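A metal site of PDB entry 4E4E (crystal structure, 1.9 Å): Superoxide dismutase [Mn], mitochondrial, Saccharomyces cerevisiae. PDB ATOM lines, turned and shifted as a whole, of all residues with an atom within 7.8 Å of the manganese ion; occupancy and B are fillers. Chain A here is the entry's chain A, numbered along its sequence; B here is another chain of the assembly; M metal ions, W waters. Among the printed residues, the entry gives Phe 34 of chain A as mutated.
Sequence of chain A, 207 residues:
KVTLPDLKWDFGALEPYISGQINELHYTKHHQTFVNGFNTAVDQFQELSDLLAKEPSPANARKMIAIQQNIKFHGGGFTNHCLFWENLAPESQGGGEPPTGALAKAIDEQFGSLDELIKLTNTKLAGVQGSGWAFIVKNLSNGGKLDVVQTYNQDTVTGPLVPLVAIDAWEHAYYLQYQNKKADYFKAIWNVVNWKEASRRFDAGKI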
ATOM      1  N   HIS A  26      28.563  -1.465   7.533  1.00  0.00           N
ATOM      2  CA  HIS A  26      27.206  -0.986   7.743  1.00  0.00           C
ATOM      3  C   HIS A  26      26.174  -1.877   7.064  1.00  0.00           C
ATOM      4  O   HIS A  26      25.118  -2.188   7.641  1.00  0.00           O
ATOM      5  CB  HIS A  26      27.106   0.428   7.178  1.00  0.00           C
ATOM      6  CG  HIS A  26      26.046   1.271   7.805  1.00  0.00           C
ATOM      7  ND1 HIS A  26      25.874   2.595   7.500  1.00  0.00           N
ATOM      8  CD2 HIS A  26      25.084   0.964   8.722  1.00  0.00           C
ATOM      9  CE1 HIS A  26      24.859   3.089   8.211  1.00  0.00           C
ATOM     10  NE2 HIS A  26      24.379   2.107   8.943  1.00  0.00           N
ATOM     11  N   TYR A  27      26.477  -2.292   5.831  1.00  0.00           N
ATOM     12  CA  TYR A  27      25.574  -3.114   5.024  1.00  0.00           C
ATOM     13  C   TYR A  27      25.680  -4.586   5.396  1.00  0.00           C
ATOM     14  O   TYR A  27      24.679  -5.230   5.730  1.00  0.00           O
ATOM     15  CB  TYR A  27      25.906  -2.930   3.543  1.00  0.00           C
ATOM     16  CG  TYR A  27      25.051  -3.707   2.565  1.00  0.00           C
ATOM     17  CD1 TYR A  27      23.760  -3.302   2.257  1.00  0.00           C
ATOM     18  CD2 TYR A  27      25.556  -4.820   1.901  1.00  0.00           C
ATOM     19  CE1 TYR A  27      22.989  -4.005   1.345  1.00  0.00           C
ATOM     20  CE2 TYR A  27      24.799  -5.528   0.990  1.00  0.00           C
ATOM     21  CZ  TYR A  27      23.508  -5.118   0.711  1.00  0.00           C
ATOM     22  OH  TYR A  27      22.733  -5.812  -0.202  1.00  0.00           O
ATOM     23  N   HIS A  30      25.749  -4.680  10.130  1.00  0.00           N
ATOM     24  CA  HIS A  30      24.605  -4.102  10.853  1.00  0.00           C
ATOM     25  C   HIS A  30      23.252  -4.418  10.196  1.00  0.00           C
ATOM     26  O   HIS A  30      22.322  -4.949  10.844  1.00  0.00           O
ATOM     27  CB  HIS A  30      24.798  -2.583  11.040  1.00  0.00           C
ATOM     28  CG  HIS A  30      26.017  -2.235  11.839  1.00  0.00           C
ATOM     29  ND1 HIS A  30      25.998  -2.165  13.217  1.00  0.00           N
ATOM     30  CD2 HIS A  30      27.272  -1.966  11.463  1.00  0.00           C
ATOM     31  CE1 HIS A  30      27.199  -1.844  13.646  1.00  0.00           C
ATOM     32  NE2 HIS A  30      28.003  -1.723  12.612  1.00  0.00           N
ATOM     33  N   HIS A  31      23.128  -4.073   8.920  1.00  0.00           N
ATOM     34  CA  HIS A  31      21.860  -4.249   8.227  1.00  0.00           C
ATOM     35  C   HIS A  31      21.484  -5.731   8.153  1.00  0.00           C
ATOM     36  O   HIS A  31      20.329  -6.088   8.356  1.00  0.00           O
ATOM     37  CB  HIS A  31      21.878  -3.623   6.840  1.00  0.00           C
ATOM     38  CG  HIS A  31      20.521  -3.377   6.276  1.00  0.00           C
ATOM     39  ND1 HIS A  31      20.302  -2.801   5.048  1.00  0.00           N
ATOM     40  CD2 HIS A  31      19.275  -3.635   6.781  1.00  0.00           C
ATOM     41  CE1 HIS A  31      19.010  -2.700   4.819  1.00  0.00           C
ATOM     42  NE2 HIS A  31      18.372  -3.212   5.858  1.00  0.00           N
ATOM     43  N   PHE A  34      19.990  -6.754  11.333  1.00  0.00           N
ATOM     44  CA  PHE A  34      18.558  -6.415  11.375  1.00  0.00           C
ATOM     45  C   PHE A  34      17.667  -7.335  10.543  1.00  0.00           C
ATOM     46  O   PHE A  34      16.584  -7.690  10.986  1.00  0.00           O
ATOM     47  CB  PHE A  34      18.325  -4.967  10.962  1.00  0.00           C
ATOM     48  CG  PHE A  34      18.882  -3.989  11.940  1.00  0.00           C
ATOM     49  CD1 PHE A  34      18.525  -4.058  13.292  1.00  0.00           C
ATOM     50  CD2 PHE A  34      19.772  -3.016  11.538  1.00  0.00           C
ATOM     51  CE1 PHE A  34      19.043  -3.133  14.199  1.00  0.00           C
ATOM     52  CE2 PHE A  34      20.290  -2.113  12.448  1.00  0.00           C
ATOM     53  CZ  PHE A  34      19.927  -2.177  13.769  1.00  0.00           C
ATOM     54  N   GLY A  77      15.137  -1.266  12.160  1.00  0.00           N
ATOM     55  CA  GLY A  77      16.471  -1.281  11.563  1.00  0.00           C
ATOM     56  C   GLY A  77      16.483  -1.682  10.096  1.00  0.00           C
ATOM     57  O   GLY A  77      17.152  -1.051   9.240  1.00  0.00           O
ATOM     58  N   ASN A  80      14.597   1.222   8.026  1.00  0.00           N
ATOM     59  CA  ASN A  80      15.349   2.488   8.038  1.00  0.00           C
ATOM     60  C   ASN A  80      16.587   2.379   7.187  1.00  0.00           C
ATOM     61  O   ASN A  80      16.881   3.294   6.402  1.00  0.00           O
ATOM     62  CB  ASN A  80      15.765   2.917   9.464  1.00  0.00           C
ATOM     63  CG  ASN A  80      14.610   3.467  10.273  1.00  0.00           C
ATOM     64  OD1 ASN A  80      13.628   3.982   9.722  1.00  0.00           O
ATOM     65  ND2 ASN A  80      14.744   3.392  11.597  1.00  0.00           N
ATOM     66  N   HIS A  81      17.328   1.268   7.314  1.00  0.00           N
ATOM     67  CA  HIS A  81      18.493   1.143   6.448  1.00  0.00           C
ATOM     68  C   HIS A  81      18.146   1.045   4.967  1.00  0.00           C
ATOM     69  O   HIS A  81      18.851   1.630   4.137  1.00  0.00           O
ATOM     70  CB  HIS A  81      19.406   0.003   6.877  1.00  0.00           C
ATOM     71  CG  HIS A  81      20.119   0.288   8.151  1.00  0.00           C
ATOM     72  ND1 HIS A  81      19.528   0.121   9.387  1.00  0.00           N
ATOM     73  CD2 HIS A  81      21.354   0.790   8.378  1.00  0.00           C
ATOM     74  CE1 HIS A  81      20.390   0.480  10.330  1.00  0.00           C
ATOM     75  NE2 HIS A  81      21.514   0.878   9.736  1.00  0.00           N
ATOM     76  N   PHE A  84      17.661   4.464   3.844  1.00  0.00           N
ATOM     77  CA  PHE A  84      18.979   5.110   3.842  1.00  0.00           C
ATOM     78  C   PHE A  84      19.747   4.830   2.560  1.00  0.00           C
ATOM     79  O   PHE A  84      20.193   5.778   1.875  1.00  0.00           O
ATOM     80  CB  PHE A  84      19.781   4.645   5.071  1.00  0.00           C
ATOM     81  CG  PHE A  84      21.013   5.469   5.358  1.00  0.00           C
ATOM     82  CD1 PHE A  84      20.941   6.860   5.423  1.00  0.00           C
ATOM     83  CD2 PHE A  84      22.224   4.847   5.612  1.00  0.00           C
ATOM     84  CE1 PHE A  84      22.083   7.617   5.714  1.00  0.00           C
ATOM     85  CE2 PHE A  84      23.358   5.599   5.904  1.00  0.00           C
ATOM     86  CZ  PHE A  84      23.289   6.979   5.951  1.00  0.00           C
ATOM     87  N   TRP A  85      19.908   3.554   2.199  1.00  0.00           N
ATOM     88  CA  TRP A  85      20.688   3.267   0.988  1.00  0.00           C
ATOM     89  C   TRP A  85      20.023   3.870  -0.217  1.00  0.00           C
ATOM     90  O   TRP A  85      20.718   4.335  -1.149  1.00  0.00           O
ATOM     91  CB  TRP A  85      20.860   1.764   0.744  1.00  0.00           C
ATOM     92  CG  TRP A  85      21.331   0.983   1.934  1.00  0.00           C
ATOM     93  CD1 TRP A  85      20.794  -0.202   2.387  1.00  0.00           C
ATOM     94  CD2 TRP A  85      22.402   1.316   2.833  1.00  0.00           C
ATOM     95  NE1 TRP A  85      21.471  -0.619   3.511  1.00  0.00           N
ATOM     96  CE2 TRP A  85      22.467   0.279   3.805  1.00  0.00           C
ATOM     97  CE3 TRP A  85      23.324   2.360   2.904  1.00  0.00           C
ATOM     98  CZ2 TRP A  85      23.401   0.281   4.843  1.00  0.00           C
ATOM     99  CZ3 TRP A  85      24.271   2.356   3.932  1.00  0.00           C
ATOM    100  CH2 TRP A  85      24.291   1.317   4.887  1.00  0.00           C
ATOM    101  N   GLY A 132      20.199   7.316  16.830  1.00  0.00           N
ATOM    102  CA  GLY A 132      18.947   7.670  16.174  1.00  0.00           C
ATOM    103  C   GLY A 132      19.049   8.082  14.726  1.00  0.00           C
ATOM    104  O   GLY A 132      20.047   7.844  14.056  1.00  0.00           O
ATOM    105  N   TRP A 133      17.987   8.737  14.258  1.00  0.00           N
ATOM    106  CA  TRP A 133      17.831   9.117  12.856  1.00  0.00           C
ATOM    107  C   TRP A 133      17.234  10.498  12.782  1.00  0.00           C
ATOM    108  O   TRP A 133      16.493  10.907  13.678  1.00  0.00           O
ATOM    109  CB  TRP A 133      16.847   8.148  12.177  1.00  0.00           C
ATOM    110  CG  TRP A 133      17.373   6.767  12.022  1.00  0.00           C
ATOM    111  CD1 TRP A 133      17.375   5.764  12.971  1.00  0.00           C
ATOM    112  CD2 TRP A 133      18.017   6.217  10.858  1.00  0.00           C
ATOM    113  NE1 TRP A 133      17.984   4.633  12.459  1.00  0.00           N
ATOM    114  CE2 TRP A 133      18.382   4.888  11.166  1.00  0.00           C
ATOM    115  CE3 TRP A 133      18.306   6.723   9.581  1.00  0.00           C
ATOM    116  CZ2 TRP A 133      19.023   4.054  10.240  1.00  0.00           C
ATOM    117  CZ3 TRP A 133      18.948   5.891   8.664  1.00  0.00           C
ATOM    118  CH2 TRP A 133      19.300   4.571   9.002  1.00  0.00           C
ATOM    119  N   ASN A 153      17.024   5.367  18.409  1.00  0.00           N
ATOM    120  CA  ASN A 153      17.255   3.951  18.169  1.00  0.00           C
ATOM    121  C   ASN A 153      16.827   3.508  16.766  1.00  0.00           C
ATOM    122  O   ASN A 153      17.337   4.065  15.786  1.00  0.00           O
ATOM    123  CB  ASN A 153      16.640   3.137  19.295  1.00  0.00           C
ATOM    124  CG  ASN A 153      17.116   3.629  20.637  1.00  0.00           C
ATOM    125  OD1 ASN A 153      18.289   3.965  20.791  1.00  0.00           O
ATOM    126  ND2 ASN A 153      16.199   3.745  21.597  1.00  0.00           N
ATOM    127  N   GLN A 154      15.970   2.501  16.646  1.00  0.00           N
ATOM    128  CA  GLN A 154      15.443   2.166  15.321  1.00  0.00           C
ATOM    129  C   GLN A 154      13.960   2.498  15.174  1.00  0.00           C
ATOM    130  O   GLN A 154      13.247   1.883  14.367  1.00  0.00           O
ATOM    131  CB  GLN A 154      15.731   0.714  14.943  1.00  0.00           C
ATOM    132  CG  GLN A 154      17.229   0.406  14.731  1.00  0.00           C
ATOM    133  CD  GLN A 154      17.873   1.264  13.647  1.00  0.00           C
ATOM    134  OE1 GLN A 154      17.188   1.801  12.768  1.00  0.00           O
ATOM    135  NE2 GLN A 154      19.202   1.417  13.713  1.00  0.00           N
ATOM    136  N   ASP A 168      21.249   8.606   9.004  1.00  0.00           N
ATOM    137  CA  ASP A 168      21.583   7.774  10.157  1.00  0.00           C
ATOM    138  C   ASP A 168      22.534   8.502  11.089  1.00  0.00           C
ATOM    139  O   ASP A 168      23.584   8.933  10.665  1.00  0.00           O
ATOM    140  CB  ASP A 168      22.322   6.541   9.656  1.00  0.00           C
ATOM    141  CG  ASP A 168      22.389   5.469  10.695  1.00  0.00           C
ATOM    142  OD1 ASP A 168      21.996   5.705  11.848  1.00  0.00           O
ATOM    143  OD2 ASP A 168      22.822   4.376  10.355  1.00  0.00           O
ATOM    144  N   ALA A 169      22.194   8.613  12.371  1.00  0.00           N
ATOM    145  CA  ALA A 169      23.126   9.263  13.295  1.00  0.00           C
ATOM    146  C   ALA A 169      23.643   8.281  14.343  1.00  0.00           C
ATOM    147  O   ALA A 169      24.204   8.703  15.359  1.00  0.00           O
ATOM    148  CB  ALA A 169      22.479  10.466  13.981  1.00  0.00           C
ATOM    149  N   TRP A 170      23.433   6.975  14.123  1.00  0.00           N
ATOM    150  CA  TRP A 170      24.130   5.987  14.963  1.00  0.00           C
ATOM    151  C   TRP A 170      25.618   6.157  14.736  1.00  0.00           C
ATOM    152  O   TRP A 170      26.044   6.436  13.601  1.00  0.00           O
ATOM    153  CB  TRP A 170      23.756   4.564  14.575  1.00  0.00           C
ATOM    154  CG  TRP A 170      22.429   4.136  15.121  1.00  0.00           C
ATOM    155  CD1 TRP A 170      21.217   4.713  14.873  1.00  0.00           C
ATOM    156  CD2 TRP A 170      22.176   3.013  15.968  1.00  0.00           C
ATOM    157  NE1 TRP A 170      20.219   4.025  15.528  1.00  0.00           N
ATOM    158  CE2 TRP A 170      20.784   2.972  16.211  1.00  0.00           C
ATOM    159  CE3 TRP A 170      22.985   2.036  16.568  1.00  0.00           C
ATOM    160  CZ2 TRP A 170      20.186   1.998  17.017  1.00  0.00           C
ATOM    161  CZ3 TRP A 170      22.391   1.074  17.362  1.00  0.00           C
ATOM    162  CH2 TRP A 170      21.007   1.056  17.581  1.00  0.00           C
ATOM    163  N   GLU A 171      26.416   5.982  15.796  1.00  0.00           N
ATOM    164  CA  GLU A 171      27.864   6.192  15.676  1.00  0.00           C
ATOM    165  C   GLU A 171      28.527   5.284  14.629  1.00  0.00           C
ATOM    166  O   GLU A 171      29.514   5.675  13.981  1.00  0.00           O
ATOM    167  CB  GLU A 171      28.545   6.083  17.055  1.00  0.00           C
ATOM    168  CG  GLU A 171      28.171   7.241  17.980  1.00  0.00           C
ATOM    169  CD  GLU A 171      28.710   7.088  19.392  1.00  0.00           C
ATOM    170  OE1 GLU A 171      28.595   5.984  19.967  1.00  0.00           O
ATOM    171  OE2 GLU A 171      29.251   8.087  19.941  1.00  0.00           O
ATOM    172  N   HIS A 172      27.970   4.098  14.414  1.00  0.00           N
ATOM    173  CA  HIS A 172      28.590   3.200  13.428  1.00  0.00           C
ATOM    174  C   HIS A 172      28.506   3.723  11.990  1.00  0.00           C
ATOM    175  O   HIS A 172      29.206   3.239  11.098  1.00  0.00           O
ATOM    176  CB  HIS A 172      28.033   1.765  13.526  1.00  0.00           C
ATOM    177  CG  HIS A 172      26.575   1.660  13.224  1.00  0.00           C
ATOM    178  ND1 HIS A 172      25.648   1.238  14.159  1.00  0.00           N
ATOM    179  CD2 HIS A 172      25.864   1.936  12.094  1.00  0.00           C
ATOM    180  CE1 HIS A 172      24.437   1.256  13.615  1.00  0.00           C
ATOM    181  NE2 HIS A 172      24.552   1.669  12.370  1.00  0.00           N
ATOM    182  N   ALA A 173      27.689   4.759  11.756  1.00  0.00           N
ATOM    183  CA  ALA A 173      27.591   5.332  10.402  1.00  0.00           C
ATOM    184  C   ALA A 173      28.774   6.247  10.069  1.00  0.00           C
ATOM    185  O   ALA A 173      28.990   6.609   8.908  1.00  0.00           O
ATOM    186  CB  ALA A 173      26.300   6.097  10.250  1.00  0.00           C
ATOM    187  N   TYR A 185      30.520  14.805   9.715  1.00  0.00           N
ATOM    188  CA  TYR A 185      29.809  13.801   8.939  1.00  0.00           C
ATOM    189  C   TYR A 185      28.437  14.317   8.495  1.00  0.00           C
ATOM    190  O   TYR A 185      28.038  14.169   7.328  1.00  0.00           O
ATOM    191  CB  TYR A 185      29.683  12.527   9.775  1.00  0.00           C
ATOM    192  CG  TYR A 185      28.558  11.596   9.389  1.00  0.00           C
ATOM    193  CD1 TYR A 185      28.624  10.816   8.244  1.00  0.00           C
ATOM    194  CD2 TYR A 185      27.432  11.462  10.194  1.00  0.00           C
ATOM    195  CE1 TYR A 185      27.595   9.950   7.895  1.00  0.00           C
ATOM    196  CE2 TYR A 185      26.400  10.608   9.863  1.00  0.00           C
ATOM    197  CZ  TYR A 185      26.479   9.846   8.715  1.00  0.00           C
ATOM    198  OH  TYR A 185      25.433   8.999   8.404  1.00  0.00           O
ATOM    199  N   GLU B 171      28.535   2.872  21.041  1.00  0.00           N
ATOM    200  CA  GLU B 171      29.473   2.402  20.046  1.00  0.00           C
ATOM    201  C   GLU B 171      30.853   3.058  20.141  1.00  0.00           C
ATOM    202  O   GLU B 171      31.865   2.417  19.839  1.00  0.00           O
ATOM    203  CB  GLU B 171      28.875   2.491  18.626  1.00  0.00           C
ATOM    204  CG  GLU B 171      27.808   1.407  18.384  1.00  0.00           C
ATOM    205  CD  GLU B 171      27.014   1.585  17.090  1.00  0.00           C
ATOM    206  OE1 GLU B 171      26.783   2.755  16.700  1.00  0.00           O
ATOM    207  OE2 GLU B 171      26.609   0.564  16.468  1.00  0.00           O
HETATM  208 MN    MN M   1      22.940   2.332  10.858  1.00  0.00          MN
HETATM  209  O   HOH W   1      21.357   2.712  12.460  1.00  0.00           O
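OD1 of Asp 168 lies within hydrogen-bond range of N of Trp 170, 3.0 Å away. A ring nitrogen (ND1) of His 172 lies within hydrogen-bond range of the side-chain carboxylate of Glu 171 of chain B (2.6 Å). A ring nitrogen (ND1) of His 81 is in hydrogen-bond range of the backbone carbonyl oxygen of Gly 77. OH of Tyr 185 sits at hydrogen-bond distance from O of Asp 168 (2.9 Å). The backbone carbonyl oxygen of His 26 sits at hydrogen-bond distance from the backbone NH of His 31 (3.0 Å).
Water W1 lies within hydrogen-bond range of NE2 of Gln 154 and OD1 of Asp 168.
Within 4 Å of the manganese ion: His 26, His 81, Asp 168 and His 172. The nearest printed residue that does not touch the manganese ion is Trp 133 (4.3 Å).
The manganese ion is bound by the side-chain carboxylate of Asp 168, water W1, a ring nitrogen (NE2) of His 172, a ring nitrogen (NE2) of His 81 and a ring nitrogen (NE2) of His 26. The manganese ion has five donor atoms within binding distance.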
